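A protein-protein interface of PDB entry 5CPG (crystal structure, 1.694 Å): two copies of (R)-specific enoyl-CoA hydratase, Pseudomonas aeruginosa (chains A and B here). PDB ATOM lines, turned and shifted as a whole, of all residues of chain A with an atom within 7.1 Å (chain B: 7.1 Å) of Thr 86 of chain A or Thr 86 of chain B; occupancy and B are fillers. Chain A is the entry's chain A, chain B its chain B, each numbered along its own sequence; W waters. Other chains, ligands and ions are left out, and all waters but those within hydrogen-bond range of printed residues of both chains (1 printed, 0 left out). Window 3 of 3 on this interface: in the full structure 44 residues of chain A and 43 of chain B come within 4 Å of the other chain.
Printed residues of chain B within 4 Å of Gln 85 of chain A: Gln 85 (3.8 Å), Thr 86 (3.5 Å) and Leu 87 (2.8 Å).
Of the printed residues of chain B, Thr 86 of chain A touches Gln 85 (3.5 Å) and Thr 86 (3.8 Å).
Of the printed residues of chain A, Gly 84 of chain B touches Leu 87 (3.2 Å).
Printed residues of chain A within 4 Å of Gln 85 of chain B: Gln 85 (3.8 Å), Thr 86 (3.5 Å) and Leu 87 (2.8 Å).
Water W1 lies within hydrogen-bond range of the side-chain hydroxyl of Thr 86 of chain A (3.1 Å), the backbone carbonyl oxygen of Leu 87 of chain B (3.2 Å) and the backbone carbonyl oxygen of Gln 85 of chain A (3.3 Å).
Hydrophobic or aromatic side chains of chain A that line the printed part of chain B: Leu 87.
Hydrophobic or aromatic side chains of chain B within 4 Å of the printed part of chain A: Leu 87.
Gly 84 of chain A touches Leu 87 of chain B, and with the chains exchanged Leu 87 of chain A touches Gly 84 of chain B.
Gln 85 of chain A touches its own counterpart, Gln 85 of chain B.
Gln 85 of chain A touches Leu 87 of chain B, and with the chains exchanged Leu 87 of chain A touches Gln 85 of chain B.
Thr 86 of chain A touches its own counterpart, Thr 86 of chain B.
The side-chain hydroxyl (OH) of Tyr 82 of chain A lies within hydrogen-bond range of the side-chain amide oxygen (OE1) of Gln 85 of chain A (2.6 Å).
The backbone NH (N) of Glu 134 of chain A is in hydrogen-bond range of the backbone carbonyl oxygen (O) of Gly 84 of chain A (2.8 Å).
NE2 of Gln 85 of chain A sits at hydrogen-bond distance from OG1 of Thr 118 of chain A (2.9 Å).
NE2 of Gln 85 of chain A is in hydrogen-bond range of O of Glu 132 of chain A (3.2 Å).
The backbone NH of Thr 86 of chain A sits at hydrogen-bond distance from the backbone carbonyl oxygen of Glu 132 of chain A (2.8 Å).
OH of Tyr 82 of chain B is in hydrogen-bond range of OE1 of Gln 85 of chain B (2.6 Å).
Among the printed residues, pairs that only touch across the chains: Gly 84 of chain A with Leu 87 of chain B, Leu 87 of chain A with Gly 84 of chain B, Gln 85 of chain A with Thr 86 of chain B, Thr 86 of chain A with Gln 85 of chain B, Thr 86 of chain A with Thr 86 of chain B and Gln 85 of chain A with Gln 85 of chain B.
The backbone NH (N) of Leu 87 of chain B lies within hydrogen-bond range of the backbone carbonyl oxygen (O) of Gln 85 of chain A, 2.8 Å away.
The backbone NH of Leu 87 of chain A sits at hydrogen-bond distance from the backbone carbonyl oxygen of Gln 85 of chain B, 2.8 Å away.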
ATOM      1  N   ILE A  67      20.495 -11.576 -27.365  1.00  0.00           N
ATOM      2  CA  ILE A  67      21.512 -12.589 -27.618  1.00  0.00           C
ATOM      3  C   ILE A  67      20.870 -13.861 -28.174  1.00  0.00           C
ATOM      4  O   ILE A  67      21.364 -14.428 -29.148  1.00  0.00           O
ATOM      5  CB  ILE A  67      22.303 -12.912 -26.340  1.00  0.00           C
ATOM      6  CG1 ILE A  67      23.278 -11.762 -26.060  1.00  0.00           C
ATOM      7  CG2 ILE A  67      23.064 -14.228 -26.477  1.00  0.00           C
ATOM      8  CD1 ILE A  67      23.898 -11.787 -24.618  1.00  0.00           C
ATOM      9  N   TYR A  82      19.637 -24.542 -28.028  1.00  0.00           N
ATOM     10  CA  TYR A  82      20.228 -23.768 -26.933  1.00  0.00           C
ATOM     11  C   TYR A  82      20.453 -24.644 -25.765  1.00  0.00           C
ATOM     12  O   TYR A  82      19.504 -25.239 -25.248  1.00  0.00           O
ATOM     13  CB  TYR A  82      19.279 -22.590 -26.646  1.00  0.00           C
ATOM     14  CG  TYR A  82      19.854 -21.264 -26.149  1.00  0.00           C
ATOM     15  CD1 TYR A  82      21.205 -21.017 -26.047  1.00  0.00           C
ATOM     16  CD2 TYR A  82      18.990 -20.216 -25.890  1.00  0.00           C
ATOM     17  CE1 TYR A  82      21.685 -19.748 -25.602  1.00  0.00           C
ATOM     18  CE2 TYR A  82      19.454 -18.955 -25.457  1.00  0.00           C
ATOM     19  CZ  TYR A  82      20.774 -18.728 -25.331  1.00  0.00           C
ATOM     20  OH  TYR A  82      21.135 -17.471 -24.912  1.00  0.00           O
ATOM     21  N   GLY A  84      22.931 -23.691 -23.057  1.00  0.00           N
ATOM     22  CA  GLY A  84      23.216 -22.910 -21.864  1.00  0.00           C
ATOM     23  C   GLY A  84      23.633 -21.491 -22.216  1.00  0.00           C
ATOM     24  O   GLY A  84      24.085 -21.225 -23.361  1.00  0.00           O
ATOM     25  N   GLN A  85      23.529 -20.603 -21.230  1.00  0.00           N
ATOM     26  CA  GLN A  85      23.951 -19.226 -21.440  1.00  0.00           C
ATOM     27  C   GLN A  85      24.429 -18.647 -20.142  1.00  0.00           C
ATOM     28  O   GLN A  85      23.744 -18.745 -19.097  1.00  0.00           O
ATOM     29  CB  GLN A  85      22.770 -18.402 -21.997  1.00  0.00           C
ATOM     30  CG  GLN A  85      23.022 -16.909 -22.096  1.00  0.00           C
ATOM     31  CD  GLN A  85      23.943 -16.577 -23.272  1.00  0.00           C
ATOM     32  OE1 GLN A  85      23.646 -16.928 -24.399  1.00  0.00           O
ATOM     33  NE2 GLN A  85      25.056 -15.885 -22.997  1.00  0.00           N
ATOM     34  N   THR A  86      25.562 -17.946 -20.216  1.00  0.00           N
ATOM     35  CA  THR A  86      26.023 -17.163 -19.083  1.00  0.00           C
ATOM     36  C   THR A  86      25.979 -15.688 -19.425  1.00  0.00           C
ATOM     37  O   THR A  86      26.277 -15.309 -20.518  1.00  0.00           O
ATOM     38  CB  THR A  86      27.437 -17.593 -18.663  1.00  0.00           C
ATOM     39  OG1 THR A  86      27.407 -18.997 -18.393  1.00  0.00           O
ATOM     40  CG2 THR A  86      27.911 -16.854 -17.421  1.00  0.00           C
ATOM     41  N   LEU A  87      25.573 -14.892 -18.468  1.00  0.00           N
ATOM     42  CA  LEU A  87      25.464 -13.451 -18.666  1.00  0.00           C
ATOM     43  C   LEU A  87      26.106 -12.711 -17.513  1.00  0.00           C
ATOM     44  O   LEU A  87      25.853 -13.004 -16.329  1.00  0.00           O
ATOM     45  CB  LEU A  87      23.982 -13.025 -18.773  1.00  0.00           C
ATOM     46  CG  LEU A  87      23.243 -13.661 -19.945  1.00  0.00           C
ATOM     47  CD1 LEU A  87      21.718 -13.475 -19.743  1.00  0.00           C
ATOM     48  CD2 LEU A  87      23.644 -12.987 -21.251  1.00  0.00           C
ATOM     49  N   ARG A  88      26.914 -11.714 -17.838  1.00  0.00           N
ATOM     50  CA  ARG A  88      27.342 -10.796 -16.776  1.00  0.00           C
ATOM     51  C   ARG A  88      26.873  -9.414 -17.207  1.00  0.00           C
ATOM     52  O   ARG A  88      27.144  -8.986 -18.331  1.00  0.00           O
ATOM     53  CB  ARG A  88      28.848 -10.854 -16.596  1.00  0.00           C
ATOM     54  CG  ARG A  88      29.324 -12.248 -16.195  1.00  0.00           C
ATOM     55  CD  ARG A  88      30.839 -12.434 -16.236  1.00  0.00           C
ATOM     56  NE  ARG A  88      31.420 -12.518 -17.589  1.00  0.00           N
ATOM     57  CZ  ARG A  88      31.477 -13.636 -18.320  1.00  0.00           C
ATOM     58  NH1 ARG A  88      30.949 -14.790 -17.888  1.00  0.00           N
ATOM     59  NH2 ARG A  88      32.044 -13.617 -19.509  1.00  0.00           N
ATOM     60  N   THR A 118      29.195 -14.106 -26.398  1.00  0.00           N
ATOM     61  CA  THR A 118      27.971 -13.326 -26.624  1.00  0.00           C
ATOM     62  C   THR A 118      28.127 -11.993 -25.912  1.00  0.00           C
ATOM     63  O   THR A 118      27.927 -11.897 -24.716  1.00  0.00           O
ATOM     64  CB  THR A 118      26.700 -14.077 -26.126  1.00  0.00           C
ATOM     65  OG1 THR A 118      26.830 -14.327 -24.723  1.00  0.00           O
ATOM     66  CG2 THR A 118      26.552 -15.423 -26.836  1.00  0.00           C
ATOM     67  N   VAL A 129      26.974  -6.094 -21.615  1.00  0.00           N
ATOM     68  CA  VAL A 129      26.852  -7.502 -21.202  1.00  0.00           C
ATOM     69  C   VAL A 129      28.014  -8.293 -21.756  1.00  0.00           C
ATOM     70  O   VAL A 129      28.423  -8.115 -22.898  1.00  0.00           O
ATOM     71  CB  VAL A 129      25.489  -8.146 -21.693  1.00  0.00           C
ATOM     72  CG1 VAL A 129      25.482  -9.661 -21.514  1.00  0.00           C
ATOM     73  CG2 VAL A 129      24.366  -7.556 -20.963  1.00  0.00           C
ATOM     74  N   ASP A 130      28.540  -9.198 -20.930  1.00  0.00           N
ATOM     75  CA  ASP A 130      29.515 -10.155 -21.391  1.00  0.00           C
ATOM     76  C   ASP A 130      28.976 -11.538 -21.089  1.00  0.00           C
ATOM     77  O   ASP A 130      28.202 -11.724 -20.149  1.00  0.00           O
ATOM     78  CB  ASP A 130      30.864  -9.939 -20.686  1.00  0.00           C
ATOM     79  CG  ASP A 130      31.981 -10.685 -21.346  1.00  0.00           C
ATOM     80  OD1 ASP A 130      31.920 -10.894 -22.578  1.00  0.00           O
ATOM     81  OD2 ASP A 130      32.910 -11.108 -20.619  1.00  0.00           O
ATOM     82  N   GLY A 131      29.401 -12.519 -21.850  1.00  0.00           N
ATOM     83  CA  GLY A 131      28.925 -13.862 -21.556  1.00  0.00           C
ATOM     84  C   GLY A 131      29.260 -14.855 -22.630  1.00  0.00           C
ATOM     85  O   GLY A 131      29.929 -14.555 -23.609  1.00  0.00           O
ATOM     86  N   GLU A 132      28.799 -16.088 -22.433  1.00  0.00           N
ATOM     87  CA  GLU A 132      29.033 -17.105 -23.424  1.00  0.00           C
ATOM     88  C   GLU A 132      27.843 -18.078 -23.481  1.00  0.00           C
ATOM     89  O   GLU A 132      27.131 -18.256 -22.490  1.00  0.00           O
ATOM     90  CB  GLU A 132      30.356 -17.844 -23.116  1.00  0.00           C
ATOM     91  CG  GLU A 132      30.578 -18.200 -21.626  1.00  0.00           C
ATOM     92  CD  GLU A 132      31.134 -17.047 -20.717  1.00  0.00           C
ATOM     93  OE1 GLU A 132      31.768 -16.081 -21.217  1.00  0.00           O
ATOM     94  OE2 GLU A 132      30.943 -17.128 -19.471  1.00  0.00           O
ATOM     95  N   ALA A 133      27.602 -18.627 -24.668  1.00  0.00           N
ATOM     96  CA  ALA A 133      26.527 -19.585 -24.883  1.00  0.00           C
ATOM     97  C   ALA A 133      27.093 -20.964 -25.204  1.00  0.00           C
ATOM     98  O   ALA A 133      28.156 -21.068 -25.825  1.00  0.00           O
ATOM     99  CB  ALA A 133      25.646 -19.125 -26.035  1.00  0.00           C
ATOM    100  N   GLU A 134      26.377 -22.018 -24.828  1.00  0.00           N
ATOM    101  CA  GLU A 134      26.696 -23.351 -25.309  1.00  0.00           C
ATOM    102  C   GLU A 134      25.488 -23.753 -26.151  1.00  0.00           C
ATOM    103  O   GLU A 134      24.337 -23.622 -25.709  1.00  0.00           O
ATOM    104  CB  GLU A 134      26.941 -24.352 -24.161  1.00  0.00           C
ATOM    105  CG  GLU A 134      27.326 -25.784 -24.672  1.00  0.00           C
ATOM    106  CD  GLU A 134      27.349 -26.863 -23.546  1.00  0.00           C
ATOM    107  OE1 GLU A 134      27.270 -26.521 -22.333  1.00  0.00           O
ATOM    108  OE2 GLU A 134      27.440 -28.068 -23.870  1.00  0.00           O
ATOM    109  N   ILE B  67      12.748 -15.748 -14.742  1.00  0.00           N
ATOM    110  CA  ILE B  67      13.692 -15.729 -13.593  1.00  0.00           C
ATOM    111  C   ILE B  67      13.992 -14.284 -13.245  1.00  0.00           C
ATOM    112  O   ILE B  67      13.972 -13.887 -12.066  1.00  0.00           O
ATOM    113  CB  ILE B  67      15.019 -16.501 -13.937  1.00  0.00           C
ATOM    114  CG1 ILE B  67      14.722 -17.993 -13.971  1.00  0.00           C
ATOM    115  CG2 ILE B  67      16.130 -16.212 -12.908  1.00  0.00           C
ATOM    116  CD1 ILE B  67      15.865 -18.823 -14.619  1.00  0.00           C
ATOM    117  N   TYR B  82      21.179  -6.668 -10.606  1.00  0.00           N
ATOM    118  CA  TYR B  82      21.466  -7.929 -11.282  1.00  0.00           C
ATOM    119  C   TYR B  82      22.877  -7.910 -11.799  1.00  0.00           C
ATOM    120  O   TYR B  82      23.212  -7.109 -12.661  1.00  0.00           O
ATOM    121  CB  TYR B  82      20.404  -8.080 -12.374  1.00  0.00           C
ATOM    122  CG  TYR B  82      19.977  -9.471 -12.818  1.00  0.00           C
ATOM    123  CD1 TYR B  82      20.411 -10.630 -12.174  1.00  0.00           C
ATOM    124  CD2 TYR B  82      19.045  -9.586 -13.842  1.00  0.00           C
ATOM    125  CE1 TYR B  82      19.973 -11.893 -12.594  1.00  0.00           C
ATOM    126  CE2 TYR B  82      18.586 -10.806 -14.274  1.00  0.00           C
ATOM    127  CZ  TYR B  82      19.042 -11.965 -13.644  1.00  0.00           C
ATOM    128  OH  TYR B  82      18.561 -13.157 -14.104  1.00  0.00           O
ATOM    129  N   GLY B  84      24.771 -11.080 -12.457  1.00  0.00           N
ATOM    130  CA  GLY B  84      25.054 -12.156 -13.374  1.00  0.00           C
ATOM    131  C   GLY B  84      23.997 -13.221 -13.330  1.00  0.00           C
ATOM    132  O   GLY B  84      23.262 -13.341 -12.343  1.00  0.00           O
ATOM    133  N   GLN B  85      23.961 -14.031 -14.387  1.00  0.00           N
ATOM    134  CA  GLN B  85      22.985 -15.111 -14.445  1.00  0.00           C
ATOM    135  C   GLN B  85      23.529 -16.249 -15.318  1.00  0.00           C
ATOM    136  O   GLN B  85      24.032 -16.010 -16.438  1.00  0.00           O
ATOM    137  CB  GLN B  85      21.631 -14.574 -14.989  1.00  0.00           C
ATOM    138  CG  GLN B  85      20.567 -15.679 -15.163  1.00  0.00           C
ATOM    139  CD  GLN B  85      19.986 -16.154 -13.867  1.00  0.00           C
ATOM    140  OE1 GLN B  85      19.434 -15.364 -13.087  1.00  0.00           O
ATOM    141  NE2 GLN B  85      20.048 -17.479 -13.646  1.00  0.00           N
ATOM    142  N   THR B  86      23.435 -17.485 -14.819  1.00  0.00           N
ATOM    143  CA  THR B  86      23.760 -18.666 -15.629  1.00  0.00           C
ATOM    144  C   THR B  86      22.483 -19.441 -15.853  1.00  0.00           C
ATOM    145  O   THR B  86      21.634 -19.478 -14.990  1.00  0.00           O
ATOM    146  CB  THR B  86      24.804 -19.588 -14.948  1.00  0.00           C
ATOM    147  OG1 THR B  86      24.245 -20.131 -13.733  1.00  0.00           O
ATOM    148  CG2 THR B  86      26.100 -18.780 -14.662  1.00  0.00           C
ATOM    149  N   LEU B  87      22.349 -20.026 -17.033  1.00  0.00           N
ATOM    150  CA  LEU B  87      21.151 -20.766 -17.396  1.00  0.00           C
ATOM    151  C   LEU B  87      21.569 -22.038 -18.086  1.00  0.00           C
ATOM    152  O   LEU B  87      22.411 -22.011 -18.974  1.00  0.00           O
ATOM    153  CB  LEU B  87      20.293 -19.930 -18.345  1.00  0.00           C
ATOM    154  CG  LEU B  87      19.769 -18.616 -17.792  1.00  0.00           C
ATOM    155  CD1 LEU B  87      19.302 -17.701 -18.951  1.00  0.00           C
ATOM    156  CD2 LEU B  87      18.615 -18.911 -16.878  1.00  0.00           C
ATOM    157  N   ARG B  88      21.007 -23.166 -17.665  1.00  0.00           N
ATOM    158  CA  ARG B  88      21.199 -24.413 -18.393  1.00  0.00           C
ATOM    159  C   ARG B  88      19.808 -24.890 -18.794  1.00  0.00           C
ATOM    160  O   ARG B  88      18.950 -25.060 -17.928  1.00  0.00           O
ATOM    161  CB  ARG B  88      21.935 -25.455 -17.528  1.00  0.00           C
ATOM    162  CG  ARG B  88      23.412 -25.082 -17.255  1.00  0.00           C
ATOM    163  CD  ARG B  88      24.116 -26.070 -16.322  1.00  0.00           C
ATOM    164  NE  ARG B  88      23.671 -25.966 -14.932  1.00  0.00           N
ATOM    165  CZ  ARG B  88      24.126 -25.080 -14.051  1.00  0.00           C
ATOM    166  NH1 ARG B  88      25.033 -24.186 -14.406  1.00  0.00           N
ATOM    167  NH2 ARG B  88      23.646 -25.064 -12.816  1.00  0.00           N
ATOM    168  N   MET B 116      22.074 -16.804  -5.702  1.00  0.00           N
ATOM    169  CA  MET B 116      20.677 -17.268  -5.692  1.00  0.00           C
ATOM    170  C   MET B 116      20.520 -18.433  -6.638  1.00  0.00           C
ATOM    171  O   MET B 116      20.915 -18.309  -7.807  1.00  0.00           O
ATOM    172  CB  MET B 116      19.712 -16.127  -6.105  1.00  0.00           C
ATOM    173  CG  MET B 116      18.233 -16.461  -5.994  1.00  0.00           C
ATOM    174  SD  MET B 116      17.556 -16.014  -4.354  1.00  0.00           S
ATOM    175  CE  MET B 116      18.233 -14.368  -4.267  1.00  0.00           C
ATOM    176  N   THR B 118      18.329 -20.506  -9.170  1.00  0.00           N
ATOM    177  CA  THR B 118      17.192 -20.066 -10.009  1.00  0.00           C
ATOM    178  C   THR B 118      16.807 -21.312 -10.816  1.00  0.00           C
ATOM    179  O   THR B 118      17.481 -21.654 -11.767  1.00  0.00           O
ATOM    180  CB  THR B 118      17.576 -18.893 -10.957  1.00  0.00           C
ATOM    181  OG1 THR B 118      18.639 -19.283 -11.817  1.00  0.00           O
ATOM    182  CG2 THR B 118      18.031 -17.691 -10.186  1.00  0.00           C
ATOM    183  N   VAL B 129      14.881 -25.606 -16.478  1.00  0.00           N
ATOM    184  CA  VAL B 129      16.048 -24.717 -16.398  1.00  0.00           C
ATOM    185  C   VAL B 129      16.742 -24.850 -15.028  1.00  0.00           C
ATOM    186  O   VAL B 129      16.084 -24.916 -13.990  1.00  0.00           O
ATOM    187  CB  VAL B 129      15.652 -23.220 -16.641  1.00  0.00           C
ATOM    188  CG1 VAL B 129      16.840 -22.292 -16.331  1.00  0.00           C
ATOM    189  CG2 VAL B 129      15.253 -23.031 -18.102  1.00  0.00           C
ATOM    190  N   ASP B 130      18.073 -24.859 -15.033  1.00  0.00           N
ATOM    191  CA  ASP B 130      18.848 -24.787 -13.804  1.00  0.00           C
ATOM    192  C   ASP B 130      19.811 -23.635 -13.956  1.00  0.00           C
ATOM    193  O   ASP B 130      20.140 -23.271 -15.088  1.00  0.00           O
ATOM    194  CB  ASP B 130      19.615 -26.097 -13.572  1.00  0.00           C
ATOM    195  CG  ASP B 130      20.183 -26.196 -12.166  1.00  0.00           C
ATOM    196  OD1 ASP B 130      19.557 -25.633 -11.252  1.00  0.00           O
ATOM    197  OD2 ASP B 130      21.241 -26.855 -12.000  1.00  0.00           O
ATOM    198  N   GLY B 131      20.226 -23.031 -12.856  1.00  0.00           N
ATOM    199  CA  GLY B 131      21.189 -21.948 -12.968  1.00  0.00           C
ATOM    200  C   GLY B 131      21.287 -21.219 -11.668  1.00  0.00           C
ATOM    201  O   GLY B 131      20.673 -21.600 -10.683  1.00  0.00           O
ATOM    202  N   GLU B 132      22.050 -20.135 -11.689  1.00  0.00           N
ATOM    203  CA  GLU B 132      22.346 -19.396 -10.497  1.00  0.00           C
ATOM    204  C   GLU B 132      22.488 -17.914 -10.892  1.00  0.00           C
ATOM    205  O   GLU B 132      23.038 -17.609 -11.974  1.00  0.00           O
ATOM    206  CB  GLU B 132      23.644 -19.923  -9.879  1.00  0.00           C
ATOM    207  CG  GLU B 132      24.089 -19.244  -8.620  1.00  0.00           C
ATOM    208  CD  GLU B 132      25.377 -19.885  -8.098  1.00  0.00           C
ATOM    209  OE1 GLU B 132      26.389 -19.162  -7.930  1.00  0.00           O
ATOM    210  OE2 GLU B 132      25.369 -21.120  -7.881  1.00  0.00           O
ATOM    211  N   ALA B 133      21.967 -17.032 -10.043  1.00  0.00           N
ATOM    212  CA  ALA B 133      22.081 -15.572 -10.244  1.00  0.00           C
ATOM    213  C   ALA B 133      23.076 -15.012  -9.242  1.00  0.00           C
ATOM    214  O   ALA B 133      23.177 -15.501  -8.117  1.00  0.00           O
ATOM    215  CB  ALA B 133      20.742 -14.886 -10.072  1.00  0.00           C
ATOM    216  N   GLU B 134      23.813 -13.996  -9.650  1.00  0.00           N
ATOM    217  CA  GLU B 134      24.620 -13.229  -8.707  1.00  0.00           C
ATOM    218  C   GLU B 134      23.972 -11.866  -8.661  1.00  0.00           C
ATOM    219  O   GLU B 134      23.704 -11.249  -9.697  1.00  0.00           O
ATOM    220  CB  GLU B 134      26.082 -13.136  -9.133  1.00  0.00           C
ATOM    221  CG  GLU B 134      26.950 -12.513  -8.046  1.00  0.00           C
ATOM    222  CD  GLU B 134      28.331 -12.144  -8.544  1.00  0.00           C
ATOM    223  OE1 GLU B 134      28.632 -12.420  -9.727  1.00  0.00           O
ATOM    224  OE2 GLU B 134      29.103 -11.558  -7.756  1.00  0.00           O
HETATM  225  O   HOH W   1      25.378 -21.313 -17.860  1.00  0.00           O
